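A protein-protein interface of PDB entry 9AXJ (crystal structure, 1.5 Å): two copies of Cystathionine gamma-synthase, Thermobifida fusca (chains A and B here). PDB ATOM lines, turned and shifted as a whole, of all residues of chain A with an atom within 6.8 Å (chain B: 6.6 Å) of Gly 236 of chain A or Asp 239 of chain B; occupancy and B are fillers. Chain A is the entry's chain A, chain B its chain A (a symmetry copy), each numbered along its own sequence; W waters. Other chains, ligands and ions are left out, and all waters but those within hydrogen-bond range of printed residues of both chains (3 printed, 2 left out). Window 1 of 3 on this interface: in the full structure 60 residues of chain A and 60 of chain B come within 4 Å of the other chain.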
ATOM      1  N   GLN A  30      -6.687  18.613  -1.087  1.00  0.00           N
ATOM      2  CA  GLN A  30      -5.378  19.128  -1.412  1.00  0.00           C
ATOM      3  C   GLN A  30      -5.308  19.345  -2.922  1.00  0.00           C
ATOM      4  O   GLN A  30      -4.806  18.531  -3.687  1.00  0.00           O
ATOM      5  CB  GLN A  30      -4.315  18.174  -0.816  1.00  0.00           C
ATOM      6  CG  GLN A  30      -2.919  18.721  -0.807  1.00  0.00           C
ATOM      7  CD  GLN A  30      -2.770  19.864   0.206  1.00  0.00           C
ATOM      8  OE1 GLN A  30      -3.121  19.736   1.367  1.00  0.00           O
ATOM      9  NE2 GLN A  30      -2.128  20.937  -0.244  1.00  0.00           N
ATOM     10  N   ASN A  53     -12.414  26.346  -0.584  1.00  0.00           N
ATOM     11  CA  ASN A  53     -11.903  24.953  -0.635  1.00  0.00           C
ATOM     12  C   ASN A  53     -12.824  24.116   0.246  1.00  0.00           C
ATOM     13  O   ASN A  53     -13.231  24.597   1.303  1.00  0.00           O
ATOM     14  CB  ASN A  53     -10.494  24.960  -0.128  1.00  0.00           C
ATOM     15  CG  ASN A  53      -9.954  23.568   0.107  1.00  0.00           C
ATOM     16  OD1 ASN A  53     -10.358  22.897   1.075  1.00  0.00           O
ATOM     17  ND2 ASN A  53      -9.054  23.107  -0.781  1.00  0.00           N
ATOM     18  N   THR A  55     -12.586  21.527   2.223  1.00  0.00           N
ATOM     19  CA  THR A  55     -12.162  21.236   3.590  1.00  0.00           C
ATOM     20  C   THR A  55     -12.257  22.551   4.427  1.00  0.00           C
ATOM     21  O   THR A  55     -12.724  22.527   5.551  1.00  0.00           O
ATOM     22  CB  THR A  55     -10.735  20.697   3.645  1.00  0.00           C
ATOM     23  OG1 THR A  55     -10.604  19.596   2.743  1.00  0.00           O
ATOM     24  CG2 THR A  55     -10.287  20.348   5.041  1.00  0.00           C
ATOM     25  N   ARG A  56     -11.781  23.657   3.878  1.00  0.00           N
ATOM     26  CA  ARG A  56     -11.848  24.954   4.597  1.00  0.00           C
ATOM     27  C   ARG A  56     -13.302  25.347   4.831  1.00  0.00           C
ATOM     28  O   ARG A  56     -13.586  25.864   5.928  1.00  0.00           O
ATOM     29  CB  ARG A  56     -11.053  26.033   3.857  1.00  0.00           C
ATOM     30  CG  ARG A  56     -10.743  27.266   4.691  1.00  0.00           C
ATOM     31  CD  ARG A  56     -10.017  28.367   3.939  1.00  0.00           C
ATOM     32  NE  ARG A  56     -10.904  29.097   3.056  1.00  0.00           N
ATOM     33  CZ  ARG A  56     -10.591  29.429   1.797  1.00  0.00           C
ATOM     34  NH1 ARG A  56      -9.547  28.886   1.189  1.00  0.00           N
ATOM     35  NH2 ARG A  56     -11.361  30.266   1.134  1.00  0.00           N
ATOM     36  N   LEU A  59     -14.595  23.641   7.993  1.00  0.00           N
ATOM     37  CA  LEU A  59     -14.080  24.323   9.219  1.00  0.00           C
ATOM     38  C   LEU A  59     -14.838  25.627   9.431  1.00  0.00           C
ATOM     39  O   LEU A  59     -15.271  25.880  10.554  1.00  0.00           O
ATOM     40  CB  LEU A  59     -12.605  24.629   9.050  1.00  0.00           C
ATOM     41  CG  LEU A  59     -11.988  25.507  10.146  1.00  0.00           C
ATOM     42  CD1 LEU A  59     -12.144  24.911  11.557  1.00  0.00           C
ATOM     43  CD2 LEU A  59     -10.533  25.790   9.857  1.00  0.00           C
ATOM     44  N   ALA A  74     -11.734  31.177   7.547  1.00  0.00           N
ATOM     45  CA  ALA A  74     -10.478  30.637   8.087  1.00  0.00           C
ATOM     46  C   ALA A  74      -9.261  31.231   7.391  1.00  0.00           C
ATOM     47  O   ALA A  74      -9.225  31.333   6.143  1.00  0.00           O
ATOM     48  CB  ALA A  74     -10.503  29.127   8.006  1.00  0.00           C
ATOM     49  N   PHE A  75      -8.222  31.504   8.180  1.00  0.00           N
ATOM     50  CA  PHE A  75      -7.044  32.254   7.744  1.00  0.00           C
ATOM     51  C   PHE A  75      -5.770  31.531   8.138  1.00  0.00           C
ATOM     52  O   PHE A  75      -5.764  30.629   9.000  1.00  0.00           O
ATOM     53  CB  PHE A  75      -7.055  33.657   8.349  1.00  0.00           C
ATOM     54  CG  PHE A  75      -8.193  34.492   7.866  1.00  0.00           C
ATOM     55  CD1 PHE A  75      -8.039  35.213   6.699  1.00  0.00           C
ATOM     56  CD2 PHE A  75      -9.435  34.466   8.488  1.00  0.00           C
ATOM     57  CE1 PHE A  75      -9.133  35.876   6.159  1.00  0.00           C
ATOM     58  CE2 PHE A  75     -10.501  35.161   7.979  1.00  0.00           C
ATOM     59  CZ  PHE A  75     -10.353  35.905   6.831  1.00  0.00           C
ATOM     60  N   ALA A  76      -4.666  31.997   7.589  1.00  0.00           N
ATOM     61  CA  ALA A  76      -3.345  31.350   7.691  1.00  0.00           C
ATOM     62  C   ALA A  76      -2.776  31.409   9.099  1.00  0.00           C
ATOM     63  O   ALA A  76      -1.836  30.672   9.437  1.00  0.00           O
ATOM     64  CB  ALA A  76      -2.370  32.079   6.769  1.00  0.00           C
ATOM     65  N   VAL A 234      -5.300  32.710   3.395  1.00  0.00           N
ATOM     66  CA  VAL A 234      -6.216  31.592   3.701  1.00  0.00           C
ATOM     67  C   VAL A 234      -5.474  30.519   4.522  1.00  0.00           C
ATOM     68  O   VAL A 234      -4.285  30.315   4.411  1.00  0.00           O
ATOM     69  CB  VAL A 234      -6.853  30.992   2.448  1.00  0.00           C
ATOM     70  CG1 VAL A 234      -7.754  32.026   1.781  1.00  0.00           C
ATOM     71  CG2 VAL A 234      -5.809  30.437   1.459  1.00  0.00           C
ATOM     72  N   ALA A 235      -6.252  29.806   5.326  1.00  0.00           N
ATOM     73  CA  ALA A 235      -5.848  28.513   5.884  1.00  0.00           C
ATOM     74  C   ALA A 235      -5.784  27.495   4.737  1.00  0.00           C
ATOM     75  O   ALA A 235      -6.752  27.333   4.015  1.00  0.00           O
ATOM     76  CB  ALA A 235      -6.811  28.051   6.937  1.00  0.00           C
ATOM     77  N   GLY A 236      -4.672  26.774   4.649  1.00  0.00           N
ATOM     78  CA  GLY A 236      -4.586  25.689   3.691  1.00  0.00           C
ATOM     79  C   GLY A 236      -5.421  24.491   4.164  1.00  0.00           C
ATOM     80  O   GLY A 236      -5.812  24.393   5.333  1.00  0.00           O
ATOM     81  N   PRO A 237      -5.795  23.591   3.242  1.00  0.00           N
ATOM     82  CA  PRO A 237      -6.746  22.548   3.568  1.00  0.00           C
ATOM     83  C   PRO A 237      -6.281  21.562   4.643  1.00  0.00           C
ATOM     84  O   PRO A 237      -7.077  21.152   5.474  1.00  0.00           O
ATOM     85  CB  PRO A 237      -7.022  21.878   2.243  1.00  0.00           C
ATOM     86  CG  PRO A 237      -5.926  22.251   1.370  1.00  0.00           C
ATOM     87  CD  PRO A 237      -5.466  23.634   1.823  1.00  0.00           C
ATOM     88  N   PHE A 238      -4.978  21.208   4.643  1.00  0.00           N
ATOM     89  CA  PHE A 238      -4.529  20.236   5.678  1.00  0.00           C
ATOM     90  C   PHE A 238      -4.538  20.900   7.051  1.00  0.00           C
ATOM     91  O   PHE A 238      -4.971  20.307   8.062  1.00  0.00           O
ATOM     92  CB  PHE A 238      -3.168  19.601   5.442  1.00  0.00           C
ATOM     93  CG  PHE A 238      -2.749  18.720   6.601  1.00  0.00           C
ATOM     94  CD1 PHE A 238      -3.469  17.574   6.938  1.00  0.00           C
ATOM     95  CD2 PHE A 238      -1.618  19.000   7.340  1.00  0.00           C
ATOM     96  CE1 PHE A 238      -3.080  16.765   7.990  1.00  0.00           C
ATOM     97  CE2 PHE A 238      -1.188  18.140   8.337  1.00  0.00           C
ATOM     98  CZ  PHE A 238      -1.893  17.012   8.654  1.00  0.00           C
ATOM     99  N   ASP A 239      -4.068  22.171   7.149  1.00  0.00           N
ATOM    100  CA  ASP A 239      -4.124  22.890   8.430  1.00  0.00           C
ATOM    101  C   ASP A 239      -5.580  23.042   8.852  1.00  0.00           C
ATOM    102  O   ASP A 239      -5.933  22.834  10.031  1.00  0.00           O
ATOM    103  CB  ASP A 239      -3.446  24.276   8.332  1.00  0.00           C
ATOM    104  CG  ASP A 239      -1.932  24.202   8.267  1.00  0.00           C
ATOM    105  OD1 ASP A 239      -1.353  23.431   9.087  1.00  0.00           O
ATOM    106  OD2 ASP A 239      -1.351  24.850   7.424  1.00  0.00           O
ATOM    107  N   ALA A 240      -6.504  23.409   7.953  1.00  0.00           N
ATOM    108  CA  ALA A 240      -7.909  23.540   8.276  1.00  0.00           C
ATOM    109  C   ALA A 240      -8.443  22.217   8.811  1.00  0.00           C
ATOM    110  O   ALA A 240      -9.224  22.203   9.771  1.00  0.00           O
ATOM    111  CB  ALA A 240      -8.684  23.963   7.061  1.00  0.00           C
ATOM    112  N   TRP A 241      -8.017  21.130   8.177  1.00  0.00           N
ATOM    113  CA  TRP A 241      -8.461  19.768   8.552  1.00  0.00           C
ATOM    114  C   TRP A 241      -7.997  19.412   9.963  1.00  0.00           C
ATOM    115  O   TRP A 241      -8.776  18.860  10.727  1.00  0.00           O
ATOM    116  CB  TRP A 241      -7.981  18.783   7.520  1.00  0.00           C
ATOM    117  CG  TRP A 241      -8.513  17.407   7.709  1.00  0.00           C
ATOM    118  CD1 TRP A 241      -9.671  16.920   7.180  1.00  0.00           C
ATOM    119  CD2 TRP A 241      -7.889  16.318   8.405  1.00  0.00           C
ATOM    120  NE1 TRP A 241      -9.835  15.619   7.530  1.00  0.00           N
ATOM    121  CE2 TRP A 241      -8.739  15.205   8.260  1.00  0.00           C
ATOM    122  CE3 TRP A 241      -6.709  16.189   9.164  1.00  0.00           C
ATOM    123  CZ2 TRP A 241      -8.442  13.985   8.844  1.00  0.00           C
ATOM    124  CZ3 TRP A 241      -6.420  14.961   9.732  1.00  0.00           C
ATOM    125  CH2 TRP A 241      -7.262  13.889   9.543  1.00  0.00           C
ATOM    126  N   ILE B  28       8.380  17.439   8.031  1.00  0.00           N
ATOM    127  CA  ILE B  28       7.206  18.352   8.109  1.00  0.00           C
ATOM    128  C   ILE B  28       7.112  18.731   9.572  1.00  0.00           C
ATOM    129  O   ILE B  28       6.706  17.911  10.408  1.00  0.00           O
ATOM    130  CB  ILE B  28       5.922  17.712   7.542  1.00  0.00           C
ATOM    131  CG1 ILE B  28       6.097  17.092   6.148  1.00  0.00           C
ATOM    132  CG2 ILE B  28       4.828  18.755   7.558  1.00  0.00           C
ATOM    133  CD1 ILE B  28       4.965  16.168   5.742  1.00  0.00           C
ATOM    134  N   GLN B  30       5.112  20.098  11.738  1.00  0.00           N
ATOM    135  CA  GLN B  30       3.732  20.398  12.034  1.00  0.00           C
ATOM    136  C   GLN B  30       3.615  20.702  13.526  1.00  0.00           C
ATOM    137  O   GLN B  30       3.258  19.868  14.349  1.00  0.00           O
ATOM    138  CB  GLN B  30       2.855  19.235  11.513  1.00  0.00           C
ATOM    139  CG  GLN B  30       1.385  19.527  11.474  1.00  0.00           C
ATOM    140  CD  GLN B  30       1.045  20.554  10.385  1.00  0.00           C
ATOM    141  OE1 GLN B  30       1.420  20.409   9.234  1.00  0.00           O
ATOM    142  NE2 GLN B  30       0.223  21.527  10.764  1.00  0.00           N
ATOM    143  N   LEU B  59      12.075  25.792   2.285  1.00  0.00           N
ATOM    144  CA  LEU B  59      11.456  26.288   1.018  1.00  0.00           C
ATOM    145  C   LEU B  59      11.977  27.687   0.712  1.00  0.00           C
ATOM    146  O   LEU B  59      12.365  27.934  -0.428  1.00  0.00           O
ATOM    147  CB  LEU B  59       9.949  26.343   1.175  1.00  0.00           C
ATOM    148  CG  LEU B  59       9.196  27.022   0.025  1.00  0.00           C
ATOM    149  CD1 LEU B  59       9.462  26.366  -1.342  1.00  0.00           C
ATOM    150  CD2 LEU B  59       7.712  27.066   0.303  1.00  0.00           C
ATOM    151  N   ALA B  76       0.838  32.294   2.173  1.00  0.00           N
ATOM    152  CA  ALA B  76      -0.350  31.421   2.124  1.00  0.00           C
ATOM    153  C   ALA B  76      -0.912  31.282   0.718  1.00  0.00           C
ATOM    154  O   ALA B  76      -1.706  30.371   0.438  1.00  0.00           O
ATOM    155  CB  ALA B  76      -1.443  32.030   3.000  1.00  0.00           C
ATOM    156  N   ASP B 207      -2.001  21.215  -6.588  1.00  0.00           N
ATOM    157  CA  ASP B 207      -2.409  20.610  -5.317  1.00  0.00           C
ATOM    158  C   ASP B 207      -1.934  21.423  -4.115  1.00  0.00           C
ATOM    159  O   ASP B 207      -2.118  20.948  -2.993  1.00  0.00           O
ATOM    160  CB  ASP B 207      -1.963  19.166  -5.236  1.00  0.00           C
ATOM    161  CG  ASP B 207      -0.476  18.927  -5.326  1.00  0.00           C
ATOM    162  OD1 ASP B 207       0.271  19.903  -5.291  1.00  0.00           O
ATOM    163  OD2 ASP B 207      -0.139  17.703  -5.445  1.00  0.00           O
ATOM    164  N   VAL B 208      -1.472  22.659  -4.271  1.00  0.00           N
ATOM    165  CA  VAL B 208      -1.048  23.479  -3.088  1.00  0.00           C
ATOM    166  C   VAL B 208      -1.024  24.966  -3.481  1.00  0.00           C
ATOM    167  O   VAL B 208      -0.176  25.362  -4.371  1.00  0.00           O
ATOM    168  CB  VAL B 208       0.304  22.985  -2.479  1.00  0.00           C
ATOM    169  CG1 VAL B 208       1.407  22.841  -3.519  1.00  0.00           C
ATOM    170  CG2 VAL B 208       0.757  23.890  -1.347  1.00  0.00           C
ATOM    171  N   VAL B 209      -1.874  25.756  -2.818  1.00  0.00           N
ATOM    172  CA  VAL B 209      -1.925  27.213  -3.056  1.00  0.00           C
ATOM    173  C   VAL B 209      -0.849  27.807  -2.170  1.00  0.00           C
ATOM    174  O   VAL B 209      -0.863  27.572  -0.971  1.00  0.00           O
ATOM    175  CB  VAL B 209      -3.319  27.743  -2.797  1.00  0.00           C
ATOM    176  CG1 VAL B 209      -3.344  29.264  -2.724  1.00  0.00           C
ATOM    177  CG2 VAL B 209      -4.335  27.235  -3.821  1.00  0.00           C
ATOM    178  N   GLY B 210      -0.021  28.649  -2.760  1.00  0.00           N
ATOM    179  CA  GLY B 210       1.057  29.273  -2.020  1.00  0.00           C
ATOM    180  C   GLY B 210       1.673  30.400  -2.798  1.00  0.00           C
ATOM    181  O   GLY B 210       1.439  30.491  -4.012  1.00  0.00           O
ATOM    182  N   ALA B 235       2.768  30.574   4.572  1.00  0.00           N
ATOM    183  CA  ALA B 235       2.600  29.195   4.107  1.00  0.00           C
ATOM    184  C   ALA B 235       2.707  28.264   5.322  1.00  0.00           C
ATOM    185  O   ALA B 235       3.684  28.323   6.048  1.00  0.00           O
ATOM    186  CB  ALA B 235       3.635  28.837   3.083  1.00  0.00           C
ATOM    187  N   GLY B 236       1.738  27.368   5.466  1.00  0.00           N
ATOM    188  CA  GLY B 236       1.836  26.352   6.497  1.00  0.00           C
ATOM    189  C   GLY B 236       2.871  25.289   6.103  1.00  0.00           C
ATOM    190  O   GLY B 236       3.280  25.181   4.940  1.00  0.00           O
ATOM    191  N   PRO B 237       3.390  24.534   7.082  1.00  0.00           N
ATOM    192  CA  PRO B 237       4.512  23.653   6.823  1.00  0.00           C
ATOM    193  C   PRO B 237       4.233  22.529   5.821  1.00  0.00           C
ATOM    194  O   PRO B 237       5.092  22.208   5.015  1.00  0.00           O
ATOM    195  CB  PRO B 237       4.892  23.135   8.189  1.00  0.00           C
ATOM    196  CG  PRO B 237       3.743  23.369   9.041  1.00  0.00           C
ATOM    197  CD  PRO B 237       3.051  24.616   8.496  1.00  0.00           C
ATOM    198  N   PHE B 238       3.011  21.954   5.854  1.00  0.00           N
ATOM    199  CA  PHE B 238       2.745  20.850   4.891  1.00  0.00           C
ATOM    200  C   PHE B 238       2.646  21.409   3.475  1.00  0.00           C
ATOM    201  O   PHE B 238       3.182  20.833   2.505  1.00  0.00           O
ATOM    202  CB  PHE B 238       1.514  20.004   5.177  1.00  0.00           C
ATOM    203  CG  PHE B 238       1.263  18.986   4.085  1.00  0.00           C
ATOM    204  CD1 PHE B 238       2.174  17.963   3.823  1.00  0.00           C
ATOM    205  CD2 PHE B 238       0.105  19.012   3.335  1.00  0.00           C
ATOM    206  CE1 PHE B 238       1.938  17.028   2.832  1.00  0.00           C
ATOM    207  CE2 PHE B 238      -0.163  18.024   2.402  1.00  0.00           C
ATOM    208  CZ  PHE B 238       0.731  17.018   2.159  1.00  0.00           C
ATOM    209  N   ASP B 239       1.962  22.569   3.293  1.00  0.00           N
ATOM    210  CA  ASP B 239       1.899  23.196   1.965  1.00  0.00           C
ATOM    211  C   ASP B 239       3.309  23.571   1.524  1.00  0.00           C
ATOM    212  O   ASP B 239       3.700  23.347   0.360  1.00  0.00           O
ATOM    213  CB  ASP B 239       0.989  24.446   1.971  1.00  0.00           C
ATOM    214  CG  ASP B 239      -0.489  24.114   2.050  1.00  0.00           C
ATOM    215  OD1 ASP B 239      -0.919  23.198   1.288  1.00  0.00           O
ATOM    216  OD2 ASP B 239      -1.179  24.706   2.850  1.00  0.00           O
ATOM    217  N   ALA B 240       4.149  24.154   2.390  1.00  0.00           N
ATOM    218  CA  ALA B 240       5.511  24.506   2.051  1.00  0.00           C
ATOM    219  C   ALA B 240       6.272  23.263   1.605  1.00  0.00           C
ATOM    220  O   ALA B 240       7.050  23.320   0.643  1.00  0.00           O
ATOM    221  CB  ALA B 240       6.194  25.141   3.228  1.00  0.00           C
ATOM    222  N   TRP B 241       6.038  22.165   2.314  1.00  0.00           N
ATOM    223  CA  TRP B 241       6.715  20.879   2.032  1.00  0.00           C
ATOM    224  C   TRP B 241       6.330  20.351   0.652  1.00  0.00           C
ATOM    225  O   TRP B 241       7.198  19.893  -0.078  1.00  0.00           O
ATOM    226  CB  TRP B 241       6.409  19.898   3.132  1.00  0.00           C
ATOM    227  CG  TRP B 241       7.174  18.626   3.035  1.00  0.00           C
ATOM    228  CD1 TRP B 241       8.396  18.387   3.590  1.00  0.00           C
ATOM    229  CD2 TRP B 241       6.754  17.400   2.419  1.00  0.00           C
ATOM    230  NE1 TRP B 241       8.787  17.113   3.328  1.00  0.00           N
ATOM    231  CE2 TRP B 241       7.785  16.466   2.636  1.00  0.00           C
ATOM    232  CE3 TRP B 241       5.619  17.015   1.678  1.00  0.00           C
ATOM    233  CZ2 TRP B 241       7.709  15.175   2.139  1.00  0.00           C
ATOM    234  CZ3 TRP B 241       5.553  15.720   1.198  1.00  0.00           C
ATOM    235  CH2 TRP B 241       6.569  14.827   1.455  1.00  0.00           C
ATOM    236  N   LEU B 242       5.066  20.439   0.293  1.00  0.00           N
ATOM    237  CA  LEU B 242       4.622  19.970  -1.036  1.00  0.00           C
ATOM    238  C   LEU B 242       5.156  20.892  -2.104  1.00  0.00           C
ATOM    239  O   LEU B 242       5.494  20.437  -3.215  1.00  0.00           O
ATOM    240  CB  LEU B 242       3.092  19.923  -1.104  1.00  0.00           C
ATOM    241  CG  LEU B 242       2.388  18.816  -0.360  1.00  0.00           C
ATOM    242  CD1 LEU B 242       0.865  19.014  -0.474  1.00  0.00           C
ATOM    243  CD2 LEU B 242       2.774  17.464  -0.950  1.00  0.00           C
ATOM    244  N   THR B 243       5.195  22.197  -1.840  1.00  0.00           N
ATOM    245  CA  THR B 243       5.764  23.151  -2.835  1.00  0.00           C
ATOM    246  C   THR B 243       7.215  22.771  -3.063  1.00  0.00           C
ATOM    247  O   THR B 243       7.691  22.656  -4.216  1.00  0.00           O
ATOM    248  CB  THR B 243       5.596  24.582  -2.298  1.00  0.00           C
ATOM    249  OG1 THR B 243       4.224  24.823  -2.038  1.00  0.00           O
ATOM    250  CG2 THR B 243       6.231  25.547  -3.290  1.00  0.00           C
ATOM    251  N   LEU B 244       7.983  22.547  -2.008  1.00  0.00           N
ATOM    252  CA  LEU B 244       9.392  22.185  -2.088  1.00  0.00           C
ATOM    253  C   LEU B 244       9.512  20.848  -2.847  1.00  0.00           C
ATOM    254  O   LEU B 244      10.400  20.698  -3.695  1.00  0.00           O
ATOM    255  CB  LEU B 244       9.947  22.065  -0.685  1.00  0.00           C
ATOM    256  CG  LEU B 244      11.424  21.883  -0.561  1.00  0.00           C
ATOM    257  CD1 LEU B 244      12.203  22.943  -1.372  1.00  0.00           C
ATOM    258  CD2 LEU B 244      11.799  21.961   0.897  1.00  0.00           C
HETATM  259  O   HOH W   1      -2.565  28.799   2.712  1.00  0.00           O
HETATM  260  O   HOH W   2      -2.833  22.009   2.947  1.00  0.00           O
HETATM  261  O   HOH W   3       0.749  22.483   7.503  1.00  0.00           O
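O of Asp 207 of chain B lies within hydrogen-bond range of NE2 of Gln 30 of chain A. The side-chain carboxylate of Asp 239 of chain B lies within hydrogen-bond range of the side-chain amide nitrogen of Gln 30 of chain A (3.0 Å). NE2 of Gln 30 of chain B sits at hydrogen-bond distance from OD1 of Asp 239 of chain A, 3.0 Å away.
The backbone carbonyl oxygen of Asp 239 of chain B is in hydrogen-bond range of the side-chain hydroxyl of Thr 243 of chain B (2.9 Å).
Among the printed residues, pairs that only touch across the chains: Gln 30 of chain A with Leu 242 of chain B (3.6 Å), Gln 30 of chain A with Phe 238 of chain B (3.6 Å), Phe 238 of chain A with Gln 30 of chain B (3.6 Å), Val 234 of chain A with Ala 76 of chain B (3.6 Å), Asp 239 of chain A with Gly 236 of chain B (3.6 Å), Gly 236 of chain A with Asp 239 of chain B (3.6 Å), Ala 76 of chain A with Ala 76 of chain B (3.9 Å), Gln 30 of chain A with Val 208 of chain B (3.9 Å) and Phe 238 of chain A with Phe 238 of chain B (3.9 Å).
Gly 236 of chain A touches just one residue of chain B: Asp 239 (3.6 Å). Asp 239 of chain B touches just these residues of chain A: Gln 30 and Gly 236. Printed residues of chain A within 4 Å of Phe 238 of chain B: Gln 30 (3.6 Å) and Phe 238 (3.9 Å). Printed residues of chain A within 4 Å of Val 208 of chain B: Gln 30 (3.9 Å). Ile 28 of chain B touches none of the printed residues of chain A. Leu 244 of chain B touches none of the printed residues of chain A.
Of the 18 printed residues of chain B, 8 touch a printed residue of chain A. Printed residues of chain A that touch a printed residue of chain B: Gln 30, Ala 76, Val 234, Gly 236, Phe 238 and Asp 239. Hydrophobic or aromatic side chains of chain A that line the printed part of chain B: Ala 76 and Phe 238. Among the printed residues, 12 pairs touch across the chains. Among the printed residues, no Asp or Glu carboxylate lies within 4 Å of a Lys or Arg side-chain nitrogen of the other chain.
Gln 30 of chain A touches Asp 239 of chain B, and with the chains exchanged Asp 239 of chain A touches Gln 30 of chain B. Ala 76 of chain B touches its own counterpart, Ala 76 of chain A. Gly 236 of chain A touches Asp 239 of chain B, and with the chains exchanged Asp 239 of chain A touches Gly 236 of chain B. Phe 238 of chain B touches its own counterpart, Phe 238 of chain A. Of the 12 pairs that touch across the chains among the printed residues, 8 have their exchanged pair printed and touching as well.
Water W2 lies within hydrogen-bond range of the side-chain amide oxygen (OE1) of Gln 30 of chain A, the side-chain carboxylate (OD1) of Asp 239 of chain B and the backbone NH (N) of Phe 238 of chain A. Water W3 lies within hydrogen-bond range of OE1 of Gln 30 of chain B (2.8 Å), OD1 of Asp 239 of chain A (2.8 Å) and N of Phe 238 of chain B (2.8 Å). Water W1 bridges the backbone carbonyl oxygen (O) of Val 234 of chain A and the backbone carbonyl oxygen (O) of Ala 76 of chain B.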
